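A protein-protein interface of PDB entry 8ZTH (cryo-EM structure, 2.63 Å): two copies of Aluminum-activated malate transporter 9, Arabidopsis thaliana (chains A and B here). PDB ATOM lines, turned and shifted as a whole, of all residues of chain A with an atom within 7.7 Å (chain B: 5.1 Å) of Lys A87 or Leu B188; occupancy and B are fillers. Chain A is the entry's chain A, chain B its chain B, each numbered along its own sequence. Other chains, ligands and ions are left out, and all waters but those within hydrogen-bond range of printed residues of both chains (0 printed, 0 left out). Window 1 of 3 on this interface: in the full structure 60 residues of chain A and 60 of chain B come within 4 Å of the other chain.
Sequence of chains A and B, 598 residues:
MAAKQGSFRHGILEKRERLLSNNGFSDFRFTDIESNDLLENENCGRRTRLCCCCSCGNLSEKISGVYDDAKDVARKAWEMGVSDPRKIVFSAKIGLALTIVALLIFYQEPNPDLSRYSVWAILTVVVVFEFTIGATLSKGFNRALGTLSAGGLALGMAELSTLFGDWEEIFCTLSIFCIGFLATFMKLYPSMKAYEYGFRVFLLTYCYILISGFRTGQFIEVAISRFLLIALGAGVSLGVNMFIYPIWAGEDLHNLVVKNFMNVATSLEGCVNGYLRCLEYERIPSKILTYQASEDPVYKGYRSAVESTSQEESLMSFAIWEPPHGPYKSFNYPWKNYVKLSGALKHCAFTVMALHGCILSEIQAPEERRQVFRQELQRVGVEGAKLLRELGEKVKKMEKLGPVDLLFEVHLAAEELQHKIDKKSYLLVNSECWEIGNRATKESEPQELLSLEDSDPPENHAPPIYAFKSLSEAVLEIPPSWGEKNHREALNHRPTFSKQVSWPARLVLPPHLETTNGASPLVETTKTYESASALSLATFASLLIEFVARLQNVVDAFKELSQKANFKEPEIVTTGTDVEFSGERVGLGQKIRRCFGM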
ATOM      1  N   MET A  80      12.651  14.561  35.527  1.00  0.00           N
ATOM      2  CA  MET A  80      13.281  14.594  34.207  1.00  0.00           C
ATOM      3  C   MET A  80      12.577  15.584  33.294  1.00  0.00           C
ATOM      4  O   MET A  80      13.200  16.156  32.395  1.00  0.00           O
ATOM      5  CB  MET A  80      13.301  13.218  33.542  1.00  0.00           C
ATOM      6  CG  MET A  80      14.458  13.074  32.546  1.00  0.00           C
ATOM      7  SD  MET A  80      14.537  11.517  31.646  1.00  0.00           S
ATOM      8  CE  MET A  80      13.257  11.772  30.420  1.00  0.00           C
ATOM      9  N   GLY A  81      11.278  15.788  33.511  1.00  0.00           N
ATOM     10  CA  GLY A  81      10.554  16.761  32.717  1.00  0.00           C
ATOM     11  C   GLY A  81      11.000  18.177  33.016  1.00  0.00           C
ATOM     12  O   GLY A  81      11.137  19.007  32.111  1.00  0.00           O
ATOM     13  N   SER A  83      13.977  19.027  34.315  1.00  0.00           N
ATOM     14  CA  SER A  83      15.368  19.208  33.903  1.00  0.00           C
ATOM     15  C   SER A  83      15.493  19.465  32.405  1.00  0.00           C
ATOM     16  O   SER A  83      16.357  20.240  31.976  1.00  0.00           O
ATOM     17  CB  SER A  83      16.195  17.987  34.302  1.00  0.00           C
ATOM     18  OG  SER A  83      15.842  16.857  33.525  1.00  0.00           O
ATOM     19  N   ASP A  84      14.656  18.825  31.591  1.00  0.00           N
ATOM     20  CA  ASP A  84      14.683  19.020  30.141  1.00  0.00           C
ATOM     21  C   ASP A  84      13.264  19.119  29.603  1.00  0.00           C
ATOM     22  O   ASP A  84      12.640  18.105  29.269  1.00  0.00           O
ATOM     23  CB  ASP A  84      15.445  17.890  29.448  1.00  0.00           C
ATOM     24  CG  ASP A  84      16.305  18.382  28.301  1.00  0.00           C
ATOM     25  OD1 ASP A  84      16.283  19.599  28.015  1.00  0.00           O
ATOM     26  OD2 ASP A  84      17.003  17.551  27.682  1.00  0.00           O
ATOM     27  N   PRO A  85      12.712  20.334  29.509  1.00  0.00           N
ATOM     28  CA  PRO A  85      11.369  20.473  28.929  1.00  0.00           C
ATOM     29  C   PRO A  85      11.328  20.179  27.441  1.00  0.00           C
ATOM     30  O   PRO A  85      10.257  20.287  26.832  1.00  0.00           O
ATOM     31  CB  PRO A  85      11.021  21.943  29.191  1.00  0.00           C
ATOM     32  CG  PRO A  85      11.855  22.352  30.341  1.00  0.00           C
ATOM     33  CD  PRO A  85      13.067  21.461  30.388  1.00  0.00           C
ATOM     34  N   ARG A  86      12.463  19.809  26.843  1.00  0.00           N
ATOM     35  CA  ARG A  86      12.510  19.446  25.435  1.00  0.00           C
ATOM     36  C   ARG A  86      11.899  18.076  25.189  1.00  0.00           C
ATOM     37  O   ARG A  86      11.479  17.785  24.065  1.00  0.00           O
ATOM     38  CB  ARG A  86      13.958  19.469  24.943  1.00  0.00           C
ATOM     39  CG  ARG A  86      14.344  20.725  24.187  1.00  0.00           C
ATOM     40  CD  ARG A  86      15.850  20.828  24.027  1.00  0.00           C
ATOM     41  NE  ARG A  86      16.476  19.524  23.845  1.00  0.00           N
ATOM     42  CZ  ARG A  86      17.453  19.276  22.984  1.00  0.00           C
ATOM     43  NH1 ARG A  86      17.946  20.225  22.205  1.00  0.00           N
ATOM     44  NH2 ARG A  86      17.950  18.045  22.903  1.00  0.00           N
ATOM     45  N   LYS A  87      11.847  17.235  26.220  1.00  0.00           N
ATOM     46  CA  LYS A  87      11.302  15.891  26.132  1.00  0.00           C
ATOM     47  C   LYS A  87       9.799  15.840  26.358  1.00  0.00           C
ATOM     48  O   LYS A  87       9.187  14.797  26.110  1.00  0.00           O
ATOM     49  CB  LYS A  87      12.002  14.987  27.151  1.00  0.00           C
ATOM     50  CG  LYS A  87      13.345  14.468  26.682  1.00  0.00           C
ATOM     51  CD  LYS A  87      14.140  13.889  27.837  1.00  0.00           C
ATOM     52  CE  LYS A  87      14.917  12.656  27.420  1.00  0.00           C
ATOM     53  NZ  LYS A  87      15.740  12.131  28.542  1.00  0.00           N
ATOM     54  N   ILE A  88       9.192  16.933  26.828  1.00  0.00           N
ATOM     55  CA  ILE A  88       7.746  16.970  27.026  1.00  0.00           C
ATOM     56  C   ILE A  88       7.006  17.503  25.810  1.00  0.00           C
ATOM     57  O   ILE A  88       5.781  17.338  25.721  1.00  0.00           O
ATOM     58  CB  ILE A  88       7.381  17.817  28.262  1.00  0.00           C
ATOM     59  CG1 ILE A  88       8.265  17.439  29.449  1.00  0.00           C
ATOM     60  CG2 ILE A  88       5.916  17.642  28.618  1.00  0.00           C
ATOM     61  CD1 ILE A  88       7.989  18.252  30.692  1.00  0.00           C
ATOM     62  N   VAL A  89       7.705  18.134  24.869  1.00  0.00           N
ATOM     63  CA  VAL A  89       7.060  18.596  23.646  1.00  0.00           C
ATOM     64  C   VAL A  89       7.105  17.530  22.554  1.00  0.00           C
ATOM     65  O   VAL A  89       6.189  17.451  21.731  1.00  0.00           O
ATOM     66  CB  VAL A  89       7.706  19.908  23.168  1.00  0.00           C
ATOM     67  CG1 VAL A  89       7.005  20.425  21.922  1.00  0.00           C
ATOM     68  CG2 VAL A  89       7.668  20.951  24.273  1.00  0.00           C
ATOM     69  N   PHE A  90       8.137  16.683  22.553  1.00  0.00           N
ATOM     70  CA  PHE A  90       8.209  15.593  21.585  1.00  0.00           C
ATOM     71  C   PHE A  90       7.051  14.617  21.772  1.00  0.00           C
ATOM     72  O   PHE A  90       6.426  14.174  20.795  1.00  0.00           O
ATOM     73  CB  PHE A  90       9.556  14.883  21.736  1.00  0.00           C
ATOM     74  CG  PHE A  90       9.884  13.936  20.619  1.00  0.00           C
ATOM     75  CD1 PHE A  90      10.018  14.395  19.322  1.00  0.00           C
ATOM     76  CD2 PHE A  90      10.078  12.591  20.871  1.00  0.00           C
ATOM     77  CE1 PHE A  90      10.326  13.526  18.297  1.00  0.00           C
ATOM     78  CE2 PHE A  90      10.385  11.719  19.849  1.00  0.00           C
ATOM     79  CZ  PHE A  90      10.509  12.187  18.562  1.00  0.00           C
ATOM     80  N   SER A  91       6.728  14.299  23.028  1.00  0.00           N
ATOM     81  CA  SER A  91       5.656  13.351  23.310  1.00  0.00           C
ATOM     82  C   SER A  91       4.301  13.923  22.920  1.00  0.00           C
ATOM     83  O   SER A  91       3.458  13.216  22.349  1.00  0.00           O
ATOM     84  CB  SER A  91       5.680  12.982  24.791  1.00  0.00           C
ATOM     85  OG  SER A  91       6.966  12.530  25.176  1.00  0.00           O
ATOM     86  N   ALA A  92       4.093  15.218  23.164  1.00  0.00           N
ATOM     87  CA  ALA A  92       2.823  15.830  22.803  1.00  0.00           C
ATOM     88  C   ALA A  92       2.709  16.022  21.300  1.00  0.00           C
ATOM     89  O   ALA A  92       1.604  15.972  20.754  1.00  0.00           O
ATOM     90  CB  ALA A  92       2.658  17.165  23.528  1.00  0.00           C
ATOM     91  N   ILE A  94       4.003  13.845  19.066  1.00  0.00           N
ATOM     92  CA  ILE A  94       3.631  12.523  18.569  1.00  0.00           C
ATOM     93  C   ILE A  94       2.161  12.237  18.856  1.00  0.00           C
ATOM     94  O   ILE A  94       1.436  11.710  17.997  1.00  0.00           O
ATOM     95  CB  ILE A  94       4.552  11.444  19.166  1.00  0.00           C
ATOM     96  CG1 ILE A  94       5.972  11.600  18.624  1.00  0.00           C
ATOM     97  CG2 ILE A  94       4.013  10.055  18.869  1.00  0.00           C
ATOM     98  CD1 ILE A  94       6.987  10.746  19.325  1.00  0.00           C
ATOM     99  N   PHE A 131      13.881  12.902  16.692  1.00  0.00           N
ATOM    100  CA  PHE A 131      14.139  14.069  17.532  1.00  0.00           C
ATOM    101  C   PHE A 131      14.525  15.313  16.735  1.00  0.00           C
ATOM    102  O   PHE A 131      14.133  16.429  17.097  1.00  0.00           O
ATOM    103  CB  PHE A 131      15.234  13.733  18.545  1.00  0.00           C
ATOM    104  CG  PHE A 131      14.976  14.274  19.920  1.00  0.00           C
ATOM    105  CD1 PHE A 131      13.898  13.832  20.663  1.00  0.00           C
ATOM    106  CD2 PHE A 131      15.818  15.226  20.468  1.00  0.00           C
ATOM    107  CE1 PHE A 131      13.660  14.332  21.924  1.00  0.00           C
ATOM    108  CE2 PHE A 131      15.586  15.728  21.730  1.00  0.00           C
ATOM    109  CZ  PHE A 131      14.505  15.281  22.460  1.00  0.00           C
ATOM    110  N   ILE A 247      13.532  21.289  16.316  1.00  0.00           N
ATOM    111  CA  ILE A 247      14.794  21.066  17.015  1.00  0.00           C
ATOM    112  C   ILE A 247      15.888  20.867  15.973  1.00  0.00           C
ATOM    113  O   ILE A 247      15.764  20.010  15.092  1.00  0.00           O
ATOM    114  CB  ILE A 247      14.713  19.859  17.964  1.00  0.00           C
ATOM    115  CG1 ILE A 247      13.867  20.200  19.191  1.00  0.00           C
ATOM    116  CG2 ILE A 247      16.104  19.419  18.383  1.00  0.00           C
ATOM    117  CD1 ILE A 247      13.873  19.125  20.250  1.00  0.00           C
ATOM    118  N   THR B 184       5.521   7.619  24.963  1.00  0.00           N
ATOM    119  CA  THR B 184       6.784   8.233  24.560  1.00  0.00           C
ATOM    120  C   THR B 184       7.583   8.702  25.774  1.00  0.00           C
ATOM    121  O   THR B 184       8.809   8.497  25.844  1.00  0.00           O
ATOM    122  CB  THR B 184       6.520   9.396  23.604  1.00  0.00           C
ATOM    123  OG1 THR B 184       5.699   8.945  22.520  1.00  0.00           O
ATOM    124  CG2 THR B 184       7.826   9.925  23.035  1.00  0.00           C
ATOM    125  N   PHE B 185       6.905   9.296  26.762  1.00  0.00           N
ATOM    126  CA  PHE B 185       7.629   9.783  27.928  1.00  0.00           C
ATOM    127  C   PHE B 185       8.279   8.626  28.672  1.00  0.00           C
ATOM    128  O   PHE B 185       9.434   8.725  29.100  1.00  0.00           O
ATOM    129  CB  PHE B 185       6.678  10.562  28.842  1.00  0.00           C
ATOM    130  CG  PHE B 185       7.374  11.451  29.840  1.00  0.00           C
ATOM    131  CD1 PHE B 185       8.120  12.540  29.419  1.00  0.00           C
ATOM    132  CD2 PHE B 185       7.264  11.209  31.198  1.00  0.00           C
ATOM    133  CE1 PHE B 185       8.753  13.362  30.335  1.00  0.00           C
ATOM    134  CE2 PHE B 185       7.895  12.027  32.116  1.00  0.00           C
ATOM    135  CZ  PHE B 185       8.641  13.103  31.686  1.00  0.00           C
ATOM    136  N   MET B 186       7.557   7.511  28.830  1.00  0.00           N
ATOM    137  CA  MET B 186       8.140   6.347  29.479  1.00  0.00           C
ATOM    138  C   MET B 186       9.236   5.707  28.637  1.00  0.00           C
ATOM    139  O   MET B 186      10.121   5.050  29.193  1.00  0.00           O
ATOM    140  CB  MET B 186       7.049   5.322  29.786  1.00  0.00           C
ATOM    141  CG  MET B 186       6.161   5.707  30.954  1.00  0.00           C
ATOM    142  SD  MET B 186       7.093   6.392  32.335  1.00  0.00           S
ATOM    143  CE  MET B 186       6.038   7.752  32.820  1.00  0.00           C
ATOM    144  N   LYS B 187       9.204   5.887  27.313  1.00  0.00           N
ATOM    145  CA  LYS B 187      10.214   5.262  26.472  1.00  0.00           C
ATOM    146  C   LYS B 187      11.497   6.076  26.405  1.00  0.00           C
ATOM    147  O   LYS B 187      12.529   5.532  26.001  1.00  0.00           O
ATOM    148  CB  LYS B 187       9.683   5.036  25.050  1.00  0.00           C
ATOM    149  CG  LYS B 187      10.751   5.162  23.960  1.00  0.00           C
ATOM    150  CD  LYS B 187      10.158   5.240  22.555  1.00  0.00           C
ATOM    151  CE  LYS B 187       9.937   3.869  21.937  1.00  0.00           C
ATOM    152  NZ  LYS B 187       9.925   3.939  20.448  1.00  0.00           N
ATOM    153  N   LEU B 188      11.477   7.339  26.840  1.00  0.00           N
ATOM    154  CA  LEU B 188      12.682   8.158  26.717  1.00  0.00           C
ATOM    155  C   LEU B 188      13.606   8.104  27.934  1.00  0.00           C
ATOM    156  O   LEU B 188      14.699   8.679  27.877  1.00  0.00           O
ATOM    157  CB  LEU B 188      12.302   9.621  26.458  1.00  0.00           C
ATOM    158  CG  LEU B 188      11.579   9.948  25.150  1.00  0.00           C
ATOM    159  CD1 LEU B 188      11.376  11.446  24.991  1.00  0.00           C
ATOM    160  CD2 LEU B 188      12.330   9.377  23.956  1.00  0.00           C
ATOM    161  N   TYR B 189      13.209   7.453  29.028  1.00  0.00           N
ATOM    162  CA  TYR B 189      14.110   7.291  30.163  1.00  0.00           C
ATOM    163  C   TYR B 189      15.286   6.359  29.866  1.00  0.00           C
ATOM    164  O   TYR B 189      15.151   5.380  29.129  1.00  0.00           O
ATOM    165  CB  TYR B 189      13.356   6.805  31.394  1.00  0.00           C
ATOM    166  CG  TYR B 189      13.020   7.927  32.338  1.00  0.00           C
ATOM    167  CD1 TYR B 189      14.028   8.518  33.086  1.00  0.00           C
ATOM    168  CD2 TYR B 189      11.716   8.360  32.532  1.00  0.00           C
ATOM    169  CE1 TYR B 189      13.764   9.521  33.973  1.00  0.00           C
ATOM    170  CE2 TYR B 189      11.442   9.385  33.417  1.00  0.00           C
ATOM    171  CZ  TYR B 189      12.476   9.956  34.131  1.00  0.00           C
ATOM    172  OH  TYR B 189      12.238  10.969  35.018  1.00  0.00           O
ATOM    173  N   PRO B 190      16.454   6.655  30.446  1.00  0.00           N
ATOM    174  CA  PRO B 190      17.658   5.857  30.159  1.00  0.00           C
ATOM    175  C   PRO B 190      17.594   4.430  30.677  1.00  0.00           C
ATOM    176  O   PRO B 190      18.186   3.534  30.062  1.00  0.00           O
ATOM    177  CB  PRO B 190      18.778   6.652  30.849  1.00  0.00           C
ATOM    178  CG  PRO B 190      18.213   8.027  31.049  1.00  0.00           C
ATOM    179  CD  PRO B 190      16.753   7.829  31.279  1.00  0.00           C
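Of the 15 printed residues of chain A, 4 touch a printed residue of chain B. Printed residues of chain A that touch a printed residue of chain B: Met A80, Lys A87, Ser A91 and Ile A94. Among the printed residues, no Asp or Glu carboxylate lies within 4 Å of a Lys or Arg side-chain nitrogen of the other chain.
Lys A87 touches one residue of chain B. Of chain A, only Lys A87 comes within 4 Å of Leu B188. Printed residues of chain A within 4 Å of Thr B184: Ser A91 and Ile A94. Of the printed residues of chain A, Tyr B189 touches Met A80. Ile A88 touches none of the printed residues of chain B. Ile A247 touches none of the printed residues of chain B. The nearest residue of chain B that does not touch Lys A87 is Phe B185 (4.1 Å). The nearest printed residue of chain B that does not touch Ile A94 is Lys B187 (7.1 Å).
The backbone carbonyl oxygen (O) of Met A80 lies within hydrogen-bond range of the side-chain hydroxyl (OG) of Ser A83 (3.0 Å). The side-chain amino group (NZ) of Lys A87 sits close to the side-chain sulfur (SD) of Met A80 (3.4 Å). The backbone carbonyl oxygen (O) of Lys A87 sits at hydrogen-bond distance from the side-chain hydroxyl (OG) of Ser A91 (3.3 Å).
No position is printed for both chains. Of the 5 pairs that touch across the chains among the printed residues, none has its exchanged pair printed and touching as well.
CB of Met A80 touches OH of Tyr B189 (2.9 Å). Lys A87 touches Leu B188. Thr B184 touches Ser A91 (CG2 to OG, 3.5 Å). Ser A91 touches Phe B185 (OG to N, 3.6 Å). CD1 of Ile A94 touches OG1 of Thr B184, 3.9 Å away.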
